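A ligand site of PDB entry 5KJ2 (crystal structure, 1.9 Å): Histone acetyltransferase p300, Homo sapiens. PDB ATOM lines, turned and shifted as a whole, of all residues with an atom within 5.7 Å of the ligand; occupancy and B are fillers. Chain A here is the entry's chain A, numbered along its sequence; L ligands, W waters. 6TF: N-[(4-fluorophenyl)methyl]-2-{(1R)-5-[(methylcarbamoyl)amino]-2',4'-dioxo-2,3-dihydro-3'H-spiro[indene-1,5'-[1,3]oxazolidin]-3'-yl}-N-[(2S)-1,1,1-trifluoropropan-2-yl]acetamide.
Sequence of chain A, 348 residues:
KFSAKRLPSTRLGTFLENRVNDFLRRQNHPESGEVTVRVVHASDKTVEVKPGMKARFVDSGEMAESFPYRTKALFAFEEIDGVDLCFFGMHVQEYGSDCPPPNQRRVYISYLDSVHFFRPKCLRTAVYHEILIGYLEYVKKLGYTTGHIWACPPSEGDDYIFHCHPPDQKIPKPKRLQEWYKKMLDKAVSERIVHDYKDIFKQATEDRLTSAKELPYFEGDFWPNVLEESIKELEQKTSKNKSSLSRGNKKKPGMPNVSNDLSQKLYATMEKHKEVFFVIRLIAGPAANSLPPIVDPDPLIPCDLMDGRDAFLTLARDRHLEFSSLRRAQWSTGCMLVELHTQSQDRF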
ATOM      1  N   PHE A  88     -26.472  -4.877  -5.105  1.00  0.00           N
ATOM      2  CA  PHE A  88     -27.492  -3.928  -4.670  1.00  0.00           C
ATOM      3  C   PHE A  88     -28.397  -4.495  -3.560  1.00  0.00           C
ATOM      4  O   PHE A  88     -28.796  -5.657  -3.616  1.00  0.00           O
ATOM      5  CB  PHE A  88     -28.367  -3.541  -5.896  1.00  0.00           C
ATOM      6  CG  PHE A  88     -29.580  -2.716  -5.600  1.00  0.00           C
ATOM      7  CD1 PHE A  88     -29.498  -1.330  -5.561  1.00  0.00           C
ATOM      8  CD2 PHE A  88     -30.810  -3.309  -5.407  1.00  0.00           C
ATOM      9  CE1 PHE A  88     -30.633  -0.558  -5.271  1.00  0.00           C
ATOM     10  CE2 PHE A  88     -31.946  -2.537  -5.117  1.00  0.00           C
ATOM     11  CZ  PHE A  88     -31.850  -1.169  -5.079  1.00  0.00           C
ATOM     12  N   LEU A 112     -30.579   2.253   0.944  1.00  0.00           N
ATOM     13  CA  LEU A 112     -30.201   1.653  -0.324  1.00  0.00           C
ATOM     14  C   LEU A 112     -28.687   1.535  -0.274  1.00  0.00           C
ATOM     15  O   LEU A 112     -28.024   2.413   0.272  1.00  0.00           O
ATOM     16  CB  LEU A 112     -30.632   2.653  -1.412  1.00  0.00           C
ATOM     17  CG  LEU A 112     -30.278   2.434  -2.871  1.00  0.00           C
ATOM     18  CD1 LEU A 112     -31.264   3.141  -3.716  1.00  0.00           C
ATOM     19  CD2 LEU A 112     -28.870   2.976  -3.197  1.00  0.00           C
ATOM     20  N   ASP A 113     -28.131   0.452  -0.827  1.00  0.00           N
ATOM     21  CA  ASP A 113     -26.685   0.233  -0.862  1.00  0.00           C
ATOM     22  C   ASP A 113     -26.308  -0.551  -2.127  1.00  0.00           C
ATOM     23  O   ASP A 113     -27.147  -1.248  -2.683  1.00  0.00           O
ATOM     24  CB  ASP A 113     -26.190  -0.501   0.392  1.00  0.00           C
ATOM     25  CG  ASP A 113     -24.713  -0.285   0.726  1.00  0.00           C
ATOM     26  OD1 ASP A 113     -23.968   0.240  -0.142  1.00  0.00           O
ATOM     27  OD2 ASP A 113     -24.299  -0.611   1.864  1.00  0.00           O
ATOM     28  N   SER A 114     -25.062  -0.393  -2.587  1.00  0.00           N
ATOM     29  CA  SER A 114     -24.536  -1.067  -3.780  1.00  0.00           C
ATOM     30  C   SER A 114     -23.045  -1.388  -3.584  1.00  0.00           C
ATOM     31  O   SER A 114     -22.372  -0.715  -2.792  1.00  0.00           O
ATOM     32  CB  SER A 114     -24.723  -0.163  -5.004  1.00  0.00           C
ATOM     33  OG  SER A 114     -24.139   1.122  -4.802  1.00  0.00           O
ATOM     34  N   ARG A 124     -23.514  -0.230 -15.346  1.00  0.00           N
ATOM     35  CA  ARG A 124     -23.922  -0.116 -13.926  1.00  0.00           C
ATOM     36  C   ARG A 124     -25.101   0.874 -13.735  1.00  0.00           C
ATOM     37  O   ARG A 124     -26.182   0.461 -13.313  1.00  0.00           O
ATOM     38  CB  ARG A 124     -22.724   0.321 -13.043  1.00  0.00           C
ATOM     39  CG  ARG A 124     -21.612  -0.709 -12.901  1.00  0.00           C
ATOM     40  CD  ARG A 124     -20.434  -0.176 -12.112  1.00  0.00           C
ATOM     41  NE  ARG A 124     -20.842   0.447 -10.846  1.00  0.00           N
ATOM     42  CZ  ARG A 124     -20.558   1.697 -10.489  1.00  0.00           C
ATOM     43  NH1 ARG A 124     -19.834   2.463 -11.290  1.00  0.00           N
ATOM     44  NH2 ARG A 124     -20.982   2.175  -9.327  1.00  0.00           N
ATOM     45  N   TYR A 128     -29.072   0.213 -12.299  1.00  0.00           N
ATOM     46  CA  TYR A 128     -29.603   0.803 -11.054  1.00  0.00           C
ATOM     47  C   TYR A 128     -30.940   1.514 -11.341  1.00  0.00           C
ATOM     48  O   TYR A 128     -31.873   1.400 -10.544  1.00  0.00           O
ATOM     49  CB  TYR A 128     -28.590   1.786 -10.448  1.00  0.00           C
ATOM     50  CG  TYR A 128     -27.267   1.216 -10.002  1.00  0.00           C
ATOM     51  CD1 TYR A 128     -27.180  -0.078  -9.469  1.00  0.00           C
ATOM     52  CD2 TYR A 128     -26.122   2.000  -9.975  1.00  0.00           C
ATOM     53  CE1 TYR A 128     -25.967  -0.586  -8.994  1.00  0.00           C
ATOM     54  CE2 TYR A 128     -24.919   1.518  -9.478  1.00  0.00           C
ATOM     55  CZ  TYR A 128     -24.841   0.215  -9.003  1.00  0.00           C
ATOM     56  OH  TYR A 128     -23.643  -0.269  -8.543  1.00  0.00           O
ATOM     57  N   HIS A 129     -31.023   2.203 -12.517  1.00  0.00           N
ATOM     58  CA  HIS A 129     -32.246   2.880 -12.964  1.00  0.00           C
ATOM     59  C   HIS A 129     -33.387   1.894 -13.122  1.00  0.00           C
ATOM     60  O   HIS A 129     -34.473   2.156 -12.619  1.00  0.00           O
ATOM     61  CB  HIS A 129     -32.037   3.674 -14.271  1.00  0.00           C
ATOM     62  CG  HIS A 129     -31.199   4.894 -14.146  1.00  0.00           C
ATOM     63  ND1 HIS A 129     -30.851   5.646 -15.263  1.00  0.00           N
ATOM     64  CD2 HIS A 129     -30.631   5.461 -13.052  1.00  0.00           C
ATOM     65  CE1 HIS A 129     -30.100   6.633 -14.808  1.00  0.00           C
ATOM     66  NE2 HIS A 129     -29.938   6.556 -13.487  1.00  0.00           N
ATOM     67  N   ILE A 131     -33.995  -1.137 -11.642  1.00  0.00           N
ATOM     68  CA  ILE A 131     -34.501  -1.583 -10.323  1.00  0.00           C
ATOM     69  C   ILE A 131     -35.380  -0.476  -9.683  1.00  0.00           C
ATOM     70  O   ILE A 131     -36.553  -0.727  -9.389  1.00  0.00           O
ATOM     71  CB  ILE A 131     -33.358  -2.031  -9.356  1.00  0.00           C
ATOM     72  CG1 ILE A 131     -32.374  -3.025 -10.019  1.00  0.00           C
ATOM     73  CG2 ILE A 131     -33.939  -2.614  -8.055  1.00  0.00           C
ATOM     74  CD1 ILE A 131     -30.969  -2.926  -9.531  1.00  0.00           C
ATOM     75  N   LEU A 132     -34.822   0.729  -9.501  1.00  0.00           N
ATOM     76  CA  LEU A 132     -35.525   1.842  -8.841  1.00  0.00           C
ATOM     77  C   LEU A 132     -36.797   2.294  -9.589  1.00  0.00           C
ATOM     78  O   LEU A 132     -37.874   2.374  -8.979  1.00  0.00           O
ATOM     79  CB  LEU A 132     -34.579   3.005  -8.547  1.00  0.00           C
ATOM     80  CG  LEU A 132     -33.431   2.746  -7.534  1.00  0.00           C
ATOM     81  CD1 LEU A 132     -32.817   4.045  -7.097  1.00  0.00           C
ATOM     82  CD2 LEU A 132     -33.907   2.004  -6.289  1.00  0.00           C
ATOM     83  N   CYS A 152     -29.188  11.128   0.519  1.00  0.00           N
ATOM     84  CA  CYS A 152     -28.130  11.486   1.463  1.00  0.00           C
ATOM     85  C   CYS A 152     -27.077  10.374   1.502  1.00  0.00           C
ATOM     86  O   CYS A 152     -27.420   9.210   1.711  1.00  0.00           O
ATOM     87  CB  CYS A 152     -28.750  11.759   2.831  1.00  0.00           C
ATOM     88  SG  CYS A 152     -27.598  11.715   4.230  1.00  0.00           S
ATOM     89  N   PRO A 153     -25.782  10.702   1.232  1.00  0.00           N
ATOM     90  CA  PRO A 153     -24.742   9.653   1.275  1.00  0.00           C
ATOM     91  C   PRO A 153     -24.341   9.327   2.720  1.00  0.00           C
ATOM     92  O   PRO A 153     -24.716  10.079   3.618  1.00  0.00           O
ATOM     93  CB  PRO A 153     -23.602  10.279   0.488  1.00  0.00           C
ATOM     94  CG  PRO A 153     -23.748  11.734   0.665  1.00  0.00           C
ATOM     95  CD  PRO A 153     -25.201  12.035   0.942  1.00  0.00           C
ATOM     96  N   PRO A 154     -23.568   8.225   2.971  1.00  0.00           N
ATOM     97  CA  PRO A 154     -23.175   7.909   4.347  1.00  0.00           C
ATOM     98  C   PRO A 154     -22.149   8.851   4.950  1.00  0.00           C
ATOM     99  O   PRO A 154     -21.439   9.559   4.222  1.00  0.00           O
ATOM    100  CB  PRO A 154     -22.626   6.486   4.227  1.00  0.00           C
ATOM    101  CG  PRO A 154     -22.072   6.420   2.856  1.00  0.00           C
ATOM    102  CD  PRO A 154     -23.038   7.224   2.025  1.00  0.00           C
ATOM    103  N   ASP A 158     -18.779   5.358   6.871  1.00  0.00           N
ATOM    104  CA  ASP A 158     -19.999   4.663   7.253  1.00  0.00           C
ATOM    105  C   ASP A 158     -20.532   3.703   6.193  1.00  0.00           C
ATOM    106  O   ASP A 158     -20.526   4.046   5.008  1.00  0.00           O
ATOM    107  CB  ASP A 158     -21.072   5.661   7.691  1.00  0.00           C
ATOM    108  CG  ASP A 158     -20.961   6.077   9.149  1.00  0.00           C
ATOM    109  OD1 ASP A 158     -19.854   6.488   9.570  1.00  0.00           O
ATOM    110  OD2 ASP A 158     -21.985   6.006   9.857  1.00  0.00           O
ATOM    111  N   ASP A 159     -20.970   2.505   6.642  1.00  0.00           N
ATOM    112  CA  ASP A 159     -21.523   1.411   5.843  1.00  0.00           C
ATOM    113  C   ASP A 159     -23.014   1.234   6.093  1.00  0.00           C
ATOM    114  O   ASP A 159     -23.428   1.170   7.250  1.00  0.00           O
ATOM    115  CB  ASP A 159     -20.750   0.097   6.112  1.00  0.00           C
ATOM    116  CG  ASP A 159     -19.375   0.015   5.481  1.00  0.00           C
ATOM    117  OD1 ASP A 159     -18.664   1.053   5.417  1.00  0.00           O
ATOM    118  OD2 ASP A 159     -19.006  -1.077   5.017  1.00  0.00           O
ATOM    119  N   TYR A 160     -23.832   1.189   5.001  1.00  0.00           N
ATOM    120  CA  TYR A 160     -25.283   1.067   5.102  1.00  0.00           C
ATOM    121  C   TYR A 160     -25.776  -0.382   5.241  1.00  0.00           C
ATOM    122  O   TYR A 160     -26.130  -0.766   6.357  1.00  0.00           O
ATOM    123  CB  TYR A 160     -26.014   1.783   3.955  1.00  0.00           C
ATOM    124  CG  TYR A 160     -26.151   3.285   4.099  1.00  0.00           C
ATOM    125  CD1 TYR A 160     -26.764   4.052   3.108  1.00  0.00           C
ATOM    126  CD2 TYR A 160     -25.676   3.954   5.227  1.00  0.00           C
ATOM    127  CE1 TYR A 160     -26.862   5.435   3.214  1.00  0.00           C
ATOM    128  CE2 TYR A 160     -25.783   5.341   5.353  1.00  0.00           C
ATOM    129  CZ  TYR A 160     -26.366   6.086   4.335  1.00  0.00           C
ATOM    130  OH  TYR A 160     -26.480   7.452   4.436  1.00  0.00           O
ATOM    131  N   HIS A 165     -16.799  -1.936   2.131  1.00  0.00           N
ATOM    132  CA  HIS A 165     -16.911  -1.633   0.713  1.00  0.00           C
ATOM    133  C   HIS A 165     -15.522  -1.569   0.045  1.00  0.00           C
ATOM    134  O   HIS A 165     -14.523  -1.441   0.755  1.00  0.00           O
ATOM    135  CB  HIS A 165     -17.675  -0.312   0.530  1.00  0.00           C
ATOM    136  CG  HIS A 165     -19.160  -0.439   0.577  1.00  0.00           C
ATOM    137  ND1 HIS A 165     -19.849  -0.463   1.785  1.00  0.00           N
ATOM    138  CD2 HIS A 165     -20.054  -0.484  -0.436  1.00  0.00           C
ATOM    139  CE1 HIS A 165     -21.126  -0.562   1.460  1.00  0.00           C
ATOM    140  NE2 HIS A 165     -21.308  -0.566   0.143  1.00  0.00           N
ATOM    141  N   PRO A 166     -15.423  -1.631  -1.318  1.00  0.00           N
ATOM    142  CA  PRO A 166     -14.104  -1.492  -1.955  1.00  0.00           C
ATOM    143  C   PRO A 166     -13.552  -0.088  -1.722  1.00  0.00           C
ATOM    144  O   PRO A 166     -14.300   0.876  -1.875  1.00  0.00           O
ATOM    145  CB  PRO A 166     -14.383  -1.729  -3.444  1.00  0.00           C
ATOM    146  CG  PRO A 166     -15.783  -2.147  -3.547  1.00  0.00           C
ATOM    147  CD  PRO A 166     -16.498  -1.741  -2.328  1.00  0.00           C
ATOM    148  N   PRO A 167     -12.256   0.061  -1.356  1.00  0.00           N
ATOM    149  CA  PRO A 167     -11.708   1.412  -1.147  1.00  0.00           C
ATOM    150  C   PRO A 167     -11.765   2.265  -2.421  1.00  0.00           C
ATOM    151  O   PRO A 167     -11.730   3.491  -2.324  1.00  0.00           O
ATOM    152  CB  PRO A 167     -10.260   1.146  -0.690  1.00  0.00           C
ATOM    153  CG  PRO A 167     -10.255  -0.278  -0.215  1.00  0.00           C
ATOM    154  CD  PRO A 167     -11.228  -0.976  -1.112  1.00  0.00           C
ATOM    155  N   GLN A 169     -14.461   2.257  -4.515  1.00  0.00           N
ATOM    156  CA  GLN A 169     -15.836   2.771  -4.548  1.00  0.00           C
ATOM    157  C   GLN A 169     -15.924   3.946  -3.585  1.00  0.00           C
ATOM    158  O   GLN A 169     -16.005   3.762  -2.370  1.00  0.00           O
ATOM    159  CB  GLN A 169     -16.844   1.670  -4.174  1.00  0.00           C
ATOM    160  CG  GLN A 169     -18.273   2.030  -4.557  1.00  0.00           C
ATOM    161  CD  GLN A 169     -19.276   1.038  -4.077  1.00  0.00           C
ATOM    162  OE1 GLN A 169     -19.040  -0.169  -4.027  1.00  0.00           O
ATOM    163  NE2 GLN A 169     -20.469   1.521  -3.748  1.00  0.00           N
ATOM    164  N   LYS A 170     -15.833   5.172  -4.129  1.00  0.00           N
ATOM    165  CA  LYS A 170     -15.855   6.395  -3.361  1.00  0.00           C
ATOM    166  C   LYS A 170     -17.253   6.728  -2.850  1.00  0.00           C
ATOM    167  O   LYS A 170     -18.252   6.433  -3.538  1.00  0.00           O
ATOM    168  CB  LYS A 170     -15.314   7.574  -4.197  1.00  0.00           C
ATOM    169  N   ILE A 171     -17.320   7.339  -1.648  1.00  0.00           N
ATOM    170  CA  ILE A 171     -18.582   7.796  -1.079  1.00  0.00           C
ATOM    171  C   ILE A 171     -18.939   9.063  -1.895  1.00  0.00           C
ATOM    172  O   ILE A 171     -18.162  10.023  -1.887  1.00  0.00           O
ATOM    173  CB  ILE A 171     -18.516   8.062   0.472  1.00  0.00           C
ATOM    174  CG1 ILE A 171     -18.366   6.745   1.261  1.00  0.00           C
ATOM    175  CG2 ILE A 171     -19.753   8.798   0.965  1.00  0.00           C
ATOM    176  CD1 ILE A 171     -16.958   6.486   1.748  1.00  0.00           C
ATOM    177  N   PRO A 172     -20.054   9.048  -2.656  1.00  0.00           N
ATOM    178  CA  PRO A 172     -20.399  10.250  -3.447  1.00  0.00           C
ATOM    179  C   PRO A 172     -20.683  11.471  -2.601  1.00  0.00           C
ATOM    180  O   PRO A 172     -21.219  11.354  -1.497  1.00  0.00           O
ATOM    181  CB  PRO A 172     -21.642   9.824  -4.213  1.00  0.00           C
ATOM    182  CG  PRO A 172     -22.246   8.750  -3.397  1.00  0.00           C
ATOM    183  CD  PRO A 172     -21.079   7.998  -2.820  1.00  0.00           C
ATOM    184  N   ARG A 176     -23.493  15.170  -6.191  1.00  0.00           N
ATOM    185  CA  ARG A 176     -23.364  14.058  -7.166  1.00  0.00           C
ATOM    186  C   ARG A 176     -24.549  13.094  -6.989  1.00  0.00           C
ATOM    187  O   ARG A 176     -25.123  12.623  -7.975  1.00  0.00           O
ATOM    188  CB  ARG A 176     -22.038  13.277  -6.958  1.00  0.00           C
ATOM    189  CG  ARG A 176     -21.873  12.128  -7.985  1.00  0.00           C
ATOM    190  CD  ARG A 176     -20.604  11.304  -7.862  1.00  0.00           C
ATOM    191  NE  ARG A 176     -20.515  10.355  -8.980  1.00  0.00           N
ATOM    192  CZ  ARG A 176     -20.210   9.061  -8.855  1.00  0.00           C
ATOM    193  NH1 ARG A 176     -19.941   8.553  -7.665  1.00  0.00           N
ATOM    194  NH2 ARG A 176     -20.177   8.284  -9.921  1.00  0.00           N
ATOM    195  N   LEU A 177     -24.873  12.758  -5.742  1.00  0.00           N
ATOM    196  CA  LEU A 177     -25.952  11.843  -5.439  1.00  0.00           C
ATOM    197  C   LEU A 177     -27.309  12.446  -5.847  1.00  0.00           C
ATOM    198  O   LEU A 177     -28.121  11.768  -6.478  1.00  0.00           O
ATOM    199  CB  LEU A 177     -25.915  11.463  -3.944  1.00  0.00           C
ATOM    200  CG  LEU A 177     -26.850  10.355  -3.485  1.00  0.00           C
ATOM    201  CD1 LEU A 177     -26.509   9.048  -4.132  1.00  0.00           C
ATOM    202  CD2 LEU A 177     -26.779  10.195  -1.985  1.00  0.00           C
ATOM    203  N   TRP A 180     -27.658  12.363  -9.512  1.00  0.00           N
ATOM    204  CA  TRP A 180     -27.970  10.993  -9.879  1.00  0.00           C
ATOM    205  C   TRP A 180     -29.462  10.696  -9.774  1.00  0.00           C
ATOM    206  O   TRP A 180     -30.027  10.070 -10.668  1.00  0.00           O
ATOM    207  CB  TRP A 180     -27.151   9.997  -9.031  1.00  0.00           C
ATOM    208  CG  TRP A 180     -27.155   8.622  -9.622  1.00  0.00           C
ATOM    209  CD1 TRP A 180     -26.231   8.100 -10.497  1.00  0.00           C
ATOM    210  CD2 TRP A 180     -28.171   7.622  -9.481  1.00  0.00           C
ATOM    211  NE1 TRP A 180     -26.614   6.841 -10.894  1.00  0.00           N
ATOM    212  CE2 TRP A 180     -27.801   6.524 -10.297  1.00  0.00           C
ATOM    213  CE3 TRP A 180     -29.371   7.538  -8.748  1.00  0.00           C
ATOM    214  CZ2 TRP A 180     -28.575   5.377 -10.389  1.00  0.00           C
ATOM    215  CZ3 TRP A 180     -30.166   6.417  -8.879  1.00  0.00           C
ATOM    216  CH2 TRP A 180     -29.777   5.354  -9.701  1.00  0.00           C
ATOM    217  N   TYR A 181     -30.086  11.034  -8.623  1.00  0.00           N
ATOM    218  CA  TYR A 181     -31.525  10.750  -8.456  1.00  0.00           C
ATOM    219  C   TYR A 181     -32.374  11.595  -9.378  1.00  0.00           C
ATOM    220  O   TYR A 181     -33.388  11.087  -9.851  1.00  0.00           O
ATOM    221  CB  TYR A 181     -31.959  10.965  -6.998  1.00  0.00           C
ATOM    222  CG  TYR A 181     -31.647   9.783  -6.107  1.00  0.00           C
ATOM    223  CD1 TYR A 181     -32.452   8.653  -6.111  1.00  0.00           C
ATOM    224  CD2 TYR A 181     -30.557   9.813  -5.235  1.00  0.00           C
ATOM    225  CE1 TYR A 181     -32.186   7.573  -5.266  1.00  0.00           C
ATOM    226  CE2 TYR A 181     -30.292   8.737  -4.376  1.00  0.00           C
ATOM    227  CZ  TYR A 181     -31.109   7.621  -4.394  1.00  0.00           C
ATOM    228  OH  TYR A 181     -30.853   6.552  -3.575  1.00  0.00           O
HETATM  229  C4  6TF L   1     -19.899   4.023  -1.496  1.00  0.00           C
HETATM  230  C5  6TF L   1     -29.285   3.602  -6.791  1.00  0.00           C
HETATM  231  C6  6TF L   1     -27.268   2.291  -6.808  1.00  0.00           C
HETATM  232  C7  6TF L   1     -20.407   2.993   0.601  1.00  0.00           C
HETATM  233  C8  6TF L   1     -22.133   3.983  -0.719  1.00  0.00           C
HETATM  234  C10 6TF L   1     -27.170   4.653  -6.433  1.00  0.00           C
HETATM  235  C13 6TF L   1     -24.369   3.959  -1.956  1.00  0.00           C
HETATM  236  C15 6TF L   1     -24.463   5.583  -4.688  1.00  0.00           C
HETATM  237  C17 6TF L   1     -22.871   3.030   1.329  1.00  0.00           C
HETATM  238  C20 6TF L   1     -24.291   5.353  -8.324  1.00  0.00           C
HETATM  239  C21 6TF L   1     -14.990   2.382   1.540  1.00  0.00           C
HETATM  240  C22 6TF L   1     -26.422   5.905  -6.180  1.00  0.00           C
HETATM  241  C24 6TF L   1     -24.024   6.093  -7.034  1.00  0.00           C
HETATM  242  C1  6TF L   1     -21.222   4.352  -1.695  1.00  0.00           C
HETATM  243  C2  6TF L   1     -28.536   4.731  -6.513  1.00  0.00           C
HETATM  244  C3  6TF L   1     -26.534   3.427  -6.564  1.00  0.00           C
HETATM  245  C9  6TF L   1     -21.731   3.325   0.415  1.00  0.00           C
HETATM  246  C11 6TF L   1     -19.474   3.361  -0.365  1.00  0.00           C
HETATM  247  C12 6TF L   1     -28.627   2.399  -6.940  1.00  0.00           C
HETATM  248  C14 6TF L   1     -24.456   6.193  -1.527  1.00  0.00           C
HETATM  249  C16 6TF L   1     -17.338   2.882   0.895  1.00  0.00           C
HETATM  250  C18 6TF L   1     -24.097   3.480   0.528  1.00  0.00           C
HETATM  251  C19 6TF L   1     -23.599   4.243  -0.705  1.00  0.00           C
HETATM  252  C23 6TF L   1     -25.511   5.397  -3.615  1.00  0.00           C
HETATM  253  C25 6TF L   1     -23.881   7.599  -7.239  1.00  0.00           C
HETATM  254  N26 6TF L   1     -24.819   5.185  -2.377  1.00  0.00           N
HETATM  255  N27 6TF L   1     -18.091   3.066  -0.262  1.00  0.00           N
HETATM  256  N28 6TF L   1     -16.018   2.632   0.559  1.00  0.00           N
HETATM  257  N29 6TF L   1     -24.982   5.768  -5.972  1.00  0.00           N
HETATM  258  O30 6TF L   1     -24.557   2.872  -2.484  1.00  0.00           O
HETATM  259  O31 6TF L   1     -24.665   7.395  -1.623  1.00  0.00           O
HETATM  260  O32 6TF L   1     -23.263   5.583  -4.428  1.00  0.00           O
HETATM  261  O33 6TF L   1     -17.757   2.904   2.052  1.00  0.00           O
HETATM  262  O34 6TF L   1     -23.788   5.643  -0.490  1.00  0.00           O
HETATM  263  F35 6TF L   1     -29.337   1.309  -7.200  1.00  0.00           F
HETATM  264  F36 6TF L   1     -22.811   7.842  -8.037  1.00  0.00           F
HETATM  265  F37 6TF L   1     -23.670   8.278  -6.094  1.00  0.00           F
HETATM  266  F38 6TF L   1     -24.951   8.205  -7.788  1.00  0.00           F
HETATM  267  O   HOH W   1     -27.368   4.784  -0.699  1.00  0.00           O
HETATM  268  O   HOH W   2     -28.499   6.629  -2.352  1.00  0.00           O
HETATM  269  O   HOH W   3     -21.140   4.042  -5.579  1.00  0.00           O
HETATM  270  O   HOH W   4     -20.243   1.935   3.370  1.00  0.00           O
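The backbone NH (N) of Ser 114 is in hydrogen-bond range of an oxygen (O30) of the ligand (3.3 Å). O30 of the ligand sits at hydrogen-bond distance from OG of Ser 114 (2.9 Å). The backbone carbonyl oxygen of Gln 169 lies within hydrogen-bond range of a nitrogen (N27) of the ligand (3.0 Å). O of Pro 166 lies within hydrogen-bond range of N28 of the ligand, 3.5 Å away.
O of Ser 114 lies within hydrogen-bond range of NE2 of Gln 169 (3.1 Å). The backbone carbonyl oxygen (O) of Ser 114 sits at hydrogen-bond distance from a ring nitrogen (NE2) of His 165, 3.1 Å away. OD1 of Asp 113 is in hydrogen-bond range of NE2 of His 165, at 2.8 Å. OD2 of Asp 159 sits at hydrogen-bond distance from ND1 of His 165, 3.4 Å away. The side-chain hydroxyl (OH) of Tyr 160 is in hydrogen-bond range of the backbone carbonyl oxygen (O) of Pro 153, 3.3 Å away. OH of Tyr 160 lies within hydrogen-bond range of O of Cys 152, 3.4 Å away.
NH1 of Arg 176 sits close to F36 of the ligand, 3.0 Å away. Residues that only touch the ligand: Trp 180, Phe 88, Pro 154, Pro 172, His 165, Asp 113, Tyr 128, Leu 177, Lys 170, Leu 132, Leu 112, Pro 153, Ile 171, Tyr 160 and Asp 159. Hydrophobic or aromatic side chains within 4 Å of the ligand: Phe 88, Leu 112, Tyr 128, Leu 132, Pro 153, Pro 154, Tyr 160, His 165, Ile 171, Pro 172, Leu 177 and Trp 180. Of the 26 residues printed, 19 come within 4 Å of the ligand.
Water W3 lies within hydrogen-bond range of O32 of the ligand and NE2 of Gln 169.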
